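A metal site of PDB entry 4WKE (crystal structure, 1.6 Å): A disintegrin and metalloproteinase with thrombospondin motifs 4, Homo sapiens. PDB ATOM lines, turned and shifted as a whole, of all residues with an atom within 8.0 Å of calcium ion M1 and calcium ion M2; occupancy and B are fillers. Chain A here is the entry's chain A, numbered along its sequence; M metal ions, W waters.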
ATOM      1  N   PHE A   7      -6.775  18.938  -5.919  1.00  0.00           N
ATOM      2  CA  PHE A   7      -6.397  17.623  -5.424  1.00  0.00           C
ATOM      3  C   PHE A   7      -6.210  17.678  -3.920  1.00  0.00           C
ATOM      4  O   PHE A   7      -5.451  18.496  -3.423  1.00  0.00           O
ATOM      5  CB  PHE A   7      -5.079  17.173  -6.063  1.00  0.00           C
ATOM      6  CG  PHE A   7      -5.107  17.222  -7.552  1.00  0.00           C
ATOM      7  CD1 PHE A   7      -4.660  18.357  -8.224  1.00  0.00           C
ATOM      8  CD2 PHE A   7      -5.608  16.161  -8.297  1.00  0.00           C
ATOM      9  CE1 PHE A   7      -4.697  18.422  -9.607  1.00  0.00           C
ATOM     10  CE2 PHE A   7      -5.646  16.226  -9.680  1.00  0.00           C
ATOM     11  CZ  PHE A   7      -5.198  17.363 -10.329  1.00  0.00           C
ATOM     12  N   VAL A   8      -6.883  16.791  -3.211  1.00  0.00           N
ATOM     13  CA  VAL A   8      -6.675  16.690  -1.769  1.00  0.00           C
ATOM     14  C   VAL A   8      -5.785  15.499  -1.475  1.00  0.00           C
ATOM     15  O   VAL A   8      -6.236  14.355  -1.574  1.00  0.00           O
ATOM     16  CB  VAL A   8      -8.007  16.502  -1.013  1.00  0.00           C
ATOM     17  CG1 VAL A   8      -7.771  16.542   0.484  1.00  0.00           C
ATOM     18  CG2 VAL A   8      -9.023  17.551  -1.413  1.00  0.00           C
ATOM     19  N   GLU A   9      -4.532  15.753  -1.103  1.00  0.00           N
ATOM     20  CA  GLU A   9      -3.597  14.690  -0.766  1.00  0.00           C
ATOM     21  C   GLU A   9      -3.929  14.172   0.623  1.00  0.00           C
ATOM     22  O   GLU A   9      -3.795  14.883   1.622  1.00  0.00           O
ATOM     23  CB  GLU A   9      -2.160  15.193  -0.834  1.00  0.00           C
ATOM     24  CG  GLU A   9      -1.765  15.674  -2.220  1.00  0.00           C
ATOM     25  CD  GLU A   9      -0.420  16.401  -2.248  1.00  0.00           C
ATOM     26  OE1 GLU A   9      -0.341  17.516  -1.727  1.00  0.00           O
ATOM     27  OE2 GLU A   9       0.568  15.871  -2.810  1.00  0.00           O
ATOM     28  N   THR A  10      -4.415  12.940   0.685  1.00  0.00           N
ATOM     29  CA  THR A  10      -5.038  12.445   1.898  1.00  0.00           C
ATOM     30  C   THR A  10      -4.231  11.355   2.602  1.00  0.00           C
ATOM     31  O   THR A  10      -3.799  10.368   1.970  1.00  0.00           O
ATOM     32  CB  THR A  10      -6.463  11.952   1.598  1.00  0.00           C
ATOM     33  OG1 THR A  10      -7.169  12.981   0.885  1.00  0.00           O
ATOM     34  CG2 THR A  10      -7.199  11.584   2.875  1.00  0.00           C
ATOM     35  N   THR A  55      -2.786   9.372  -0.588  1.00  0.00           N
ATOM     36  CA  THR A  55      -1.340   9.382  -0.814  1.00  0.00           C
ATOM     37  C   THR A  55      -0.541   8.653   0.243  1.00  0.00           C
ATOM     38  O   THR A  55       0.590   8.243  -0.033  1.00  0.00           O
ATOM     39  CB  THR A  55      -0.830  10.821  -0.932  1.00  0.00           C
ATOM     40  OG1 THR A  55      -1.177  11.535   0.271  1.00  0.00           O
ATOM     41  CG2 THR A  55      -1.452  11.503  -2.140  1.00  0.00           C
ATOM     42  N   THR A  89       4.974  16.890   6.981  1.00  0.00           N
ATOM     43  CA  THR A  89       6.168  17.682   6.732  1.00  0.00           C
ATOM     44  C   THR A  89       5.790  19.148   6.605  1.00  0.00           C
ATOM     45  O   THR A  89       4.620  19.477   6.383  1.00  0.00           O
ATOM     46  CB  THR A  89       6.890  17.216   5.459  1.00  0.00           C
ATOM     47  OG1 THR A  89       5.990  17.349   4.346  1.00  0.00           O
ATOM     48  CG2 THR A  89       7.352  15.781   5.581  1.00  0.00           C
ATOM     49  N   GLU A  91       6.365  21.434   4.259  1.00  0.00           N
ATOM     50  CA  GLU A  91       6.083  21.981   2.923  1.00  0.00           C
ATOM     51  C   GLU A  91       5.305  21.033   2.012  1.00  0.00           C
ATOM     52  O   GLU A  91       5.633  19.853   1.890  1.00  0.00           O
ATOM     53  CB  GLU A  91       7.408  22.376   2.254  1.00  0.00           C
ATOM     54  CG  GLU A  91       8.201  23.396   3.041  1.00  0.00           C
ATOM     55  CD  GLU A  91       7.468  24.715   3.221  1.00  0.00           C
ATOM     56  OE1 GLU A  91       6.563  25.015   2.404  1.00  0.00           O
ATOM     57  OE2 GLU A  91       7.793  25.472   4.167  1.00  0.00           O
ATOM     58  N   ASP A  92       4.303  21.583   1.333  1.00  0.00           N
ATOM     59  CA  ASP A  92       3.444  20.805   0.430  1.00  0.00           C
ATOM     60  C   ASP A  92       4.207  20.238  -0.765  1.00  0.00           C
ATOM     61  O   ASP A  92       3.775  19.257  -1.370  1.00  0.00           O
ATOM     62  CB  ASP A  92       2.264  21.657  -0.034  1.00  0.00           C
ATOM     63  CG  ASP A  92       1.040  20.844  -0.444  1.00  0.00           C
ATOM     64  OD1 ASP A  92       1.088  19.617  -0.513  1.00  0.00           O
ATOM     65  OD2 ASP A  92      -0.002  21.470  -0.688  1.00  0.00           O
ATOM     66  N   SER A  93       5.341  20.841  -1.103  1.00  0.00           N
ATOM     67  CA  SER A  93       6.167  20.332  -2.194  1.00  0.00           C
ATOM     68  C   SER A  93       6.943  19.056  -1.847  1.00  0.00           C
ATOM     69  O   SER A  93       7.440  18.371  -2.749  1.00  0.00           O
ATOM     70  CB  SER A  93       7.132  21.421  -2.671  1.00  0.00           C
ATOM     71  OG  SER A  93       7.924  21.902  -1.601  1.00  0.00           O
ATOM     72  N   ASP A  94       7.055  18.746  -0.557  1.00  0.00           N
ATOM     73  CA  ASP A  94       7.627  17.477  -0.102  1.00  0.00           C
ATOM     74  C   ASP A  94       6.615  16.384  -0.418  1.00  0.00           C
ATOM     75  O   ASP A  94       5.449  16.531  -0.052  1.00  0.00           O
ATOM     76  CB  ASP A  94       7.870  17.547   1.407  1.00  0.00           C
ATOM     77  CG  ASP A  94       8.552  16.312   1.960  1.00  0.00           C
ATOM     78  OD1 ASP A  94       8.160  15.169   1.621  1.00  0.00           O
ATOM     79  OD2 ASP A  94       9.477  16.483   2.771  1.00  0.00           O
ATOM     80  N   PRO A  95       7.036  15.296  -1.089  1.00  0.00           N
ATOM     81  CA  PRO A  95       6.092  14.242  -1.487  1.00  0.00           C
ATOM     82  C   PRO A  95       5.374  13.576  -0.293  1.00  0.00           C
ATOM     83  O   PRO A  95       4.265  13.063  -0.484  1.00  0.00           O
ATOM     84  CB  PRO A  95       6.980  13.221  -2.218  1.00  0.00           C
ATOM     85  CG  PRO A  95       8.357  13.477  -1.714  1.00  0.00           C
ATOM     86  CD  PRO A  95       8.420  14.963  -1.491  1.00  0.00           C
ATOM     87  N   ASP A  96       5.978  13.589   0.888  1.00  0.00           N
ATOM     88  CA  ASP A  96       5.367  12.992   2.084  1.00  0.00           C
ATOM     89  C   ASP A  96       4.301  13.896   2.703  1.00  0.00           C
ATOM     90  O   ASP A  96       3.563  13.479   3.610  1.00  0.00           O
ATOM     91  CB  ASP A  96       6.410  12.691   3.176  1.00  0.00           C
ATOM     92  CG  ASP A  96       7.362  11.570   2.805  1.00  0.00           C
ATOM     93  OD1 ASP A  96       7.108  10.804   1.852  1.00  0.00           O
ATOM     94  OD2 ASP A  96       8.395  11.442   3.512  1.00  0.00           O
ATOM     95  N   HIS A  97       4.222  15.151   2.255  1.00  0.00           N
ATOM     96  CA  HIS A  97       3.235  16.064   2.811  1.00  0.00           C
ATOM     97  C   HIS A  97       1.837  15.634   2.429  1.00  0.00           C
ATOM     98  O   HIS A  97       1.614  15.159   1.313  1.00  0.00           O
ATOM     99  CB  HIS A  97       3.468  17.494   2.314  1.00  0.00           C
ATOM    100  CG  HIS A  97       2.575  18.501   2.966  1.00  0.00           C
ATOM    101  ND1 HIS A  97       2.898  19.120   4.152  1.00  0.00           N
ATOM    102  CD2 HIS A  97       1.351  18.970   2.610  1.00  0.00           C
ATOM    103  CE1 HIS A  97       1.923  19.940   4.498  1.00  0.00           C
ATOM    104  NE2 HIS A  97       0.976  19.876   3.574  1.00  0.00           N
ATOM    105  N   PHE A  98       0.895  15.825   3.346  1.00  0.00           N
ATOM    106  CA  PHE A  98      -0.522  15.572   3.048  1.00  0.00           C
ATOM    107  C   PHE A  98      -1.367  16.774   3.466  1.00  0.00           C
ATOM    108  O   PHE A  98      -0.965  17.560   4.335  1.00  0.00           O
ATOM    109  CB  PHE A  98      -1.027  14.282   3.717  1.00  0.00           C
ATOM    110  CG  PHE A  98      -0.729  14.182   5.182  1.00  0.00           C
ATOM    111  CD1 PHE A  98      -1.634  14.643   6.135  1.00  0.00           C
ATOM    112  CD2 PHE A  98       0.460  13.621   5.632  1.00  0.00           C
ATOM    113  CE1 PHE A  98      -1.357  14.540   7.488  1.00  0.00           C
ATOM    114  CE2 PHE A  98       0.731  13.498   6.972  1.00  0.00           C
ATOM    115  CZ  PHE A  98      -0.176  13.978   7.910  1.00  0.00           C
ATOM    116  N   ASP A  99      -2.499  16.916   2.797  1.00  0.00           N
ATOM    117  CA  ASP A  99      -3.428  18.045   2.998  1.00  0.00           C
ATOM    118  C   ASP A  99      -4.538  17.786   4.013  1.00  0.00           C
ATOM    119  O   ASP A  99      -5.102  18.742   4.568  1.00  0.00           O
ATOM    120  CB  ASP A  99      -4.102  18.425   1.670  1.00  0.00           C
ATOM    121  CG  ASP A  99      -3.129  18.816   0.570  1.00  0.00           C
ATOM    122  OD1 ASP A  99      -2.160  19.539   0.846  1.00  0.00           O
ATOM    123  OD2 ASP A  99      -3.347  18.419  -0.585  1.00  0.00           O
ATOM    124  N   THR A 100      -4.896  16.527   4.234  1.00  0.00           N
ATOM    125  CA  THR A 100      -5.909  16.205   5.227  1.00  0.00           C
ATOM    126  C   THR A 100      -5.654  14.803   5.747  1.00  0.00           C
ATOM    127  O   THR A 100      -5.005  13.993   5.073  1.00  0.00           O
ATOM    128  CB  THR A 100      -7.338  16.364   4.652  1.00  0.00           C
ATOM    129  OG1 THR A 100      -8.276  16.581   5.715  1.00  0.00           O
ATOM    130  CG2 THR A 100      -7.751  15.188   3.807  1.00  0.00           C
ATOM    131  N   VAL A 126      -9.310  22.712   5.573  1.00  0.00           N
ATOM    132  CA  VAL A 126      -8.609  21.792   4.654  1.00  0.00           C
ATOM    133  C   VAL A 126      -7.137  22.132   4.429  1.00  0.00           C
ATOM    134  O   VAL A 126      -6.319  21.229   4.282  1.00  0.00           O
ATOM    135  CB  VAL A 126      -9.355  21.594   3.306  1.00  0.00           C
ATOM    136  CG1 VAL A 126      -9.111  22.747   2.335  1.00  0.00           C
ATOM    137  CG2 VAL A 126      -8.956  20.268   2.660  1.00  0.00           C
ATOM    138  N   CYS A 127      -6.794  23.412   4.389  1.00  0.00           N
ATOM    139  CA  CYS A 127      -5.405  23.811   4.137  1.00  0.00           C
ATOM    140  C   CYS A 127      -4.689  24.368   5.364  1.00  0.00           C
ATOM    141  O   CYS A 127      -3.727  25.123   5.248  1.00  0.00           O
ATOM    142  CB  CYS A 127      -5.325  24.779   2.955  1.00  0.00           C
ATOM    143  SG  CYS A 127      -5.713  23.948   1.407  1.00  0.00           S
ATOM    144  N   GLY A 209      -8.454  27.012  -0.328  1.00  0.00           N
ATOM    145  CA  GLY A 209      -7.974  25.771  -0.919  1.00  0.00           C
ATOM    146  C   GLY A 209      -6.639  25.921  -1.625  1.00  0.00           C
ATOM    147  O   GLY A 209      -6.363  25.188  -2.568  1.00  0.00           O
ATOM    148  N   HIS A 210      -5.810  26.840  -1.159  1.00  0.00           N
ATOM    149  CA  HIS A 210      -4.527  27.140  -1.806  1.00  0.00           C
ATOM    150  C   HIS A 210      -3.553  25.965  -1.798  1.00  0.00           C
ATOM    151  O   HIS A 210      -2.604  25.942  -2.572  1.00  0.00           O
ATOM    152  CB  HIS A 210      -3.859  28.348  -1.161  1.00  0.00           C
ATOM    153  CG  HIS A 210      -3.632  28.185   0.297  1.00  0.00           C
ATOM    154  ND1 HIS A 210      -2.534  27.537   0.822  1.00  0.00           N
ATOM    155  CD2 HIS A 210      -4.388  28.544   1.361  1.00  0.00           C
ATOM    156  CE1 HIS A 210      -2.616  27.522   2.138  1.00  0.00           C
ATOM    157  NE2 HIS A 210      -3.736  28.127   2.489  1.00  0.00           N
ATOM    158  N   CYS A 211      -3.790  24.988  -0.922  1.00  0.00           N
ATOM    159  CA  CYS A 211      -2.930  23.810  -0.825  1.00  0.00           C
ATOM    160  C   CYS A 211      -3.420  22.662  -1.691  1.00  0.00           C
ATOM    161  O   CYS A 211      -2.842  21.583  -1.648  1.00  0.00           O
ATOM    162  CB  CYS A 211      -2.825  23.348   0.624  1.00  0.00           C
ATOM    163  SG  CYS A 211      -4.281  22.493   1.253  1.00  0.00           S
ATOM    164  N   LEU A 212      -4.475  22.879  -2.474  1.00  0.00           N
ATOM    165  CA  LEU A 212      -5.055  21.825  -3.260  1.00  0.00           C
ATOM    166  C   LEU A 212      -4.674  21.921  -4.724  1.00  0.00           C
ATOM    167  O   LEU A 212      -5.245  21.225  -5.578  1.00  0.00           O
ATOM    168  CB  LEU A 212      -6.577  21.878  -3.137  1.00  0.00           C
ATOM    169  CG  LEU A 212      -7.115  21.828  -1.713  1.00  0.00           C
ATOM    170  CD1 LEU A 212      -8.629  21.962  -1.764  1.00  0.00           C
ATOM    171  CD2 LEU A 212      -6.697  20.550  -0.986  1.00  0.00           C
ATOM    172  N   LEU A 213      -3.680  22.763  -5.036  1.00  0.00           N
ATOM    173  CA  LEU A 213      -3.366  23.040  -6.430  1.00  0.00           C
ATOM    174  C   LEU A 213      -2.276  22.156  -7.004  1.00  0.00           C
ATOM    175  O   LEU A 213      -2.162  22.071  -8.225  1.00  0.00           O
ATOM    176  CB  LEU A 213      -2.999  24.511  -6.614  1.00  0.00           C
ATOM    177  CG  LEU A 213      -3.989  25.553  -6.096  1.00  0.00           C
ATOM    178  CD1 LEU A 213      -3.484  26.953  -6.403  1.00  0.00           C
ATOM    179  CD2 LEU A 213      -5.363  25.351  -6.705  1.00  0.00           C
ATOM    180  N   ASP A 214      -1.461  21.535  -6.154  1.00  0.00           N
ATOM    181  CA  ASP A 214      -0.386  20.668  -6.613  1.00  0.00           C
ATOM    182  C   ASP A 214      -0.871  19.230  -6.822  1.00  0.00           C
ATOM    183  O   ASP A 214      -1.663  18.712  -6.045  1.00  0.00           O
ATOM    184  CB  ASP A 214       0.836  20.733  -5.672  1.00  0.00           C
ATOM    185  CG  ASP A 214       0.546  20.232  -4.252  1.00  0.00           C
ATOM    186  OD1 ASP A 214      -0.489  20.588  -3.650  1.00  0.00           O
ATOM    187  OD2 ASP A 214       1.405  19.500  -3.718  1.00  0.00           O
ATOM    188  N   LYS A 215      -0.423  18.602  -7.903  1.00  0.00           N
ATOM    189  CA  LYS A 215      -0.843  17.251  -8.246  1.00  0.00           C
ATOM    190  C   LYS A 215       0.023  16.247  -7.487  1.00  0.00           C
ATOM    191  O   LYS A 215       1.241  16.408  -7.429  1.00  0.00           O
ATOM    192  CB  LYS A 215      -0.718  17.039  -9.765  1.00  0.00           C
ATOM    193  CG  LYS A 215      -1.784  16.148 -10.378  1.00  0.00           C
ATOM    194  CD  LYS A 215      -2.005  16.542 -11.835  1.00  0.00           C
ATOM    195  CE  LYS A 215      -2.692  15.459 -12.639  1.00  0.00           C
ATOM    196  NZ  LYS A 215      -1.758  14.342 -12.975  1.00  0.00           N
ATOM    197  N   PRO A 216      -0.589  15.207  -6.877  1.00  0.00           N
ATOM    198  CA  PRO A 216       0.225  14.217  -6.168  1.00  0.00           C
ATOM    199  C   PRO A 216       1.035  13.344  -7.114  1.00  0.00           C
ATOM    200  O   PRO A 216       0.598  13.054  -8.225  1.00  0.00           O
ATOM    201  CB  PRO A 216      -0.805  13.371  -5.422  1.00  0.00           C
ATOM    202  CG  PRO A 216      -2.072  13.573  -6.167  1.00  0.00           C
ATOM    203  CD  PRO A 216      -2.021  14.983  -6.666  1.00  0.00           C
ATOM    204  N   GLU A 217       2.203  12.917  -6.646  1.00  0.00           N
ATOM    205  CA  GLU A 217       3.157  12.147  -7.461  1.00  0.00           C
ATOM    206  C   GLU A 217       2.820  10.659  -7.531  1.00  0.00           C
ATOM    207  O   GLU A 217       3.019  10.020  -8.570  1.00  0.00           O
ATOM    208  CB  GLU A 217       4.563  12.314  -6.876  1.00  0.00           C
HETATM  209 CA    CA M   1       1.932  17.979  -2.162  1.00  0.00          CA
HETATM  210 CA    CA M   2      -1.472  19.673  -1.583  1.00  0.00          CA
HETATM  211  O   HOH W   1      -2.713  18.836  -3.491  1.00  0.00           O
HETATM  212  O   HOH W   2       2.879  16.262  -0.809  1.00  0.00           O
HETATM  213  O   HOH W   3       3.250  17.188  -3.974  1.00  0.00           O
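N of Thr 100 is in hydrogen-bond range of O of Glu 9, 3.3 Å away. The side-chain sulfur (SG) of Cys 127 forms a disulfide with the side-chain sulfur (SG) of Cys 211 (2.0 Å).
Along chain A the residues within 4 Å of calcium ion M1 span positions 9 to 214.
Of the 27 residues printed, 5 come within 4 Å of calcium ion M2.
Calcium ion M1 is bound by OD2 of Asp 214, OE1 of Glu 9, water W3, O of Asp 92, water W2, OD1 of Asp 92 and OE2 of Glu 9.
Calcium ion M2 is bound by the backbone carbonyl oxygen (O) of Cys 211 (2.4 Å), water W1 (2.4 Å), the side-chain carboxylate (OE1) of Glu 9 (2.4 Å), the side-chain carboxylate (OD1) of Asp 214 (2.5 Å), the side-chain carboxylate (OD2) of Asp 99 (2.5 Å), the side-chain carboxylate (OD2) of Asp 92 (2.5 Å), the side-chain carboxylate (OD1) of Asp 99 (2.5 Å) and the side-chain carboxylate (OD1) of Asp 92 (2.8 Å).
Water W1 bridges the backbone carbonyl oxygen of Phe 7 and the backbone carbonyl oxygen of Asp 214.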
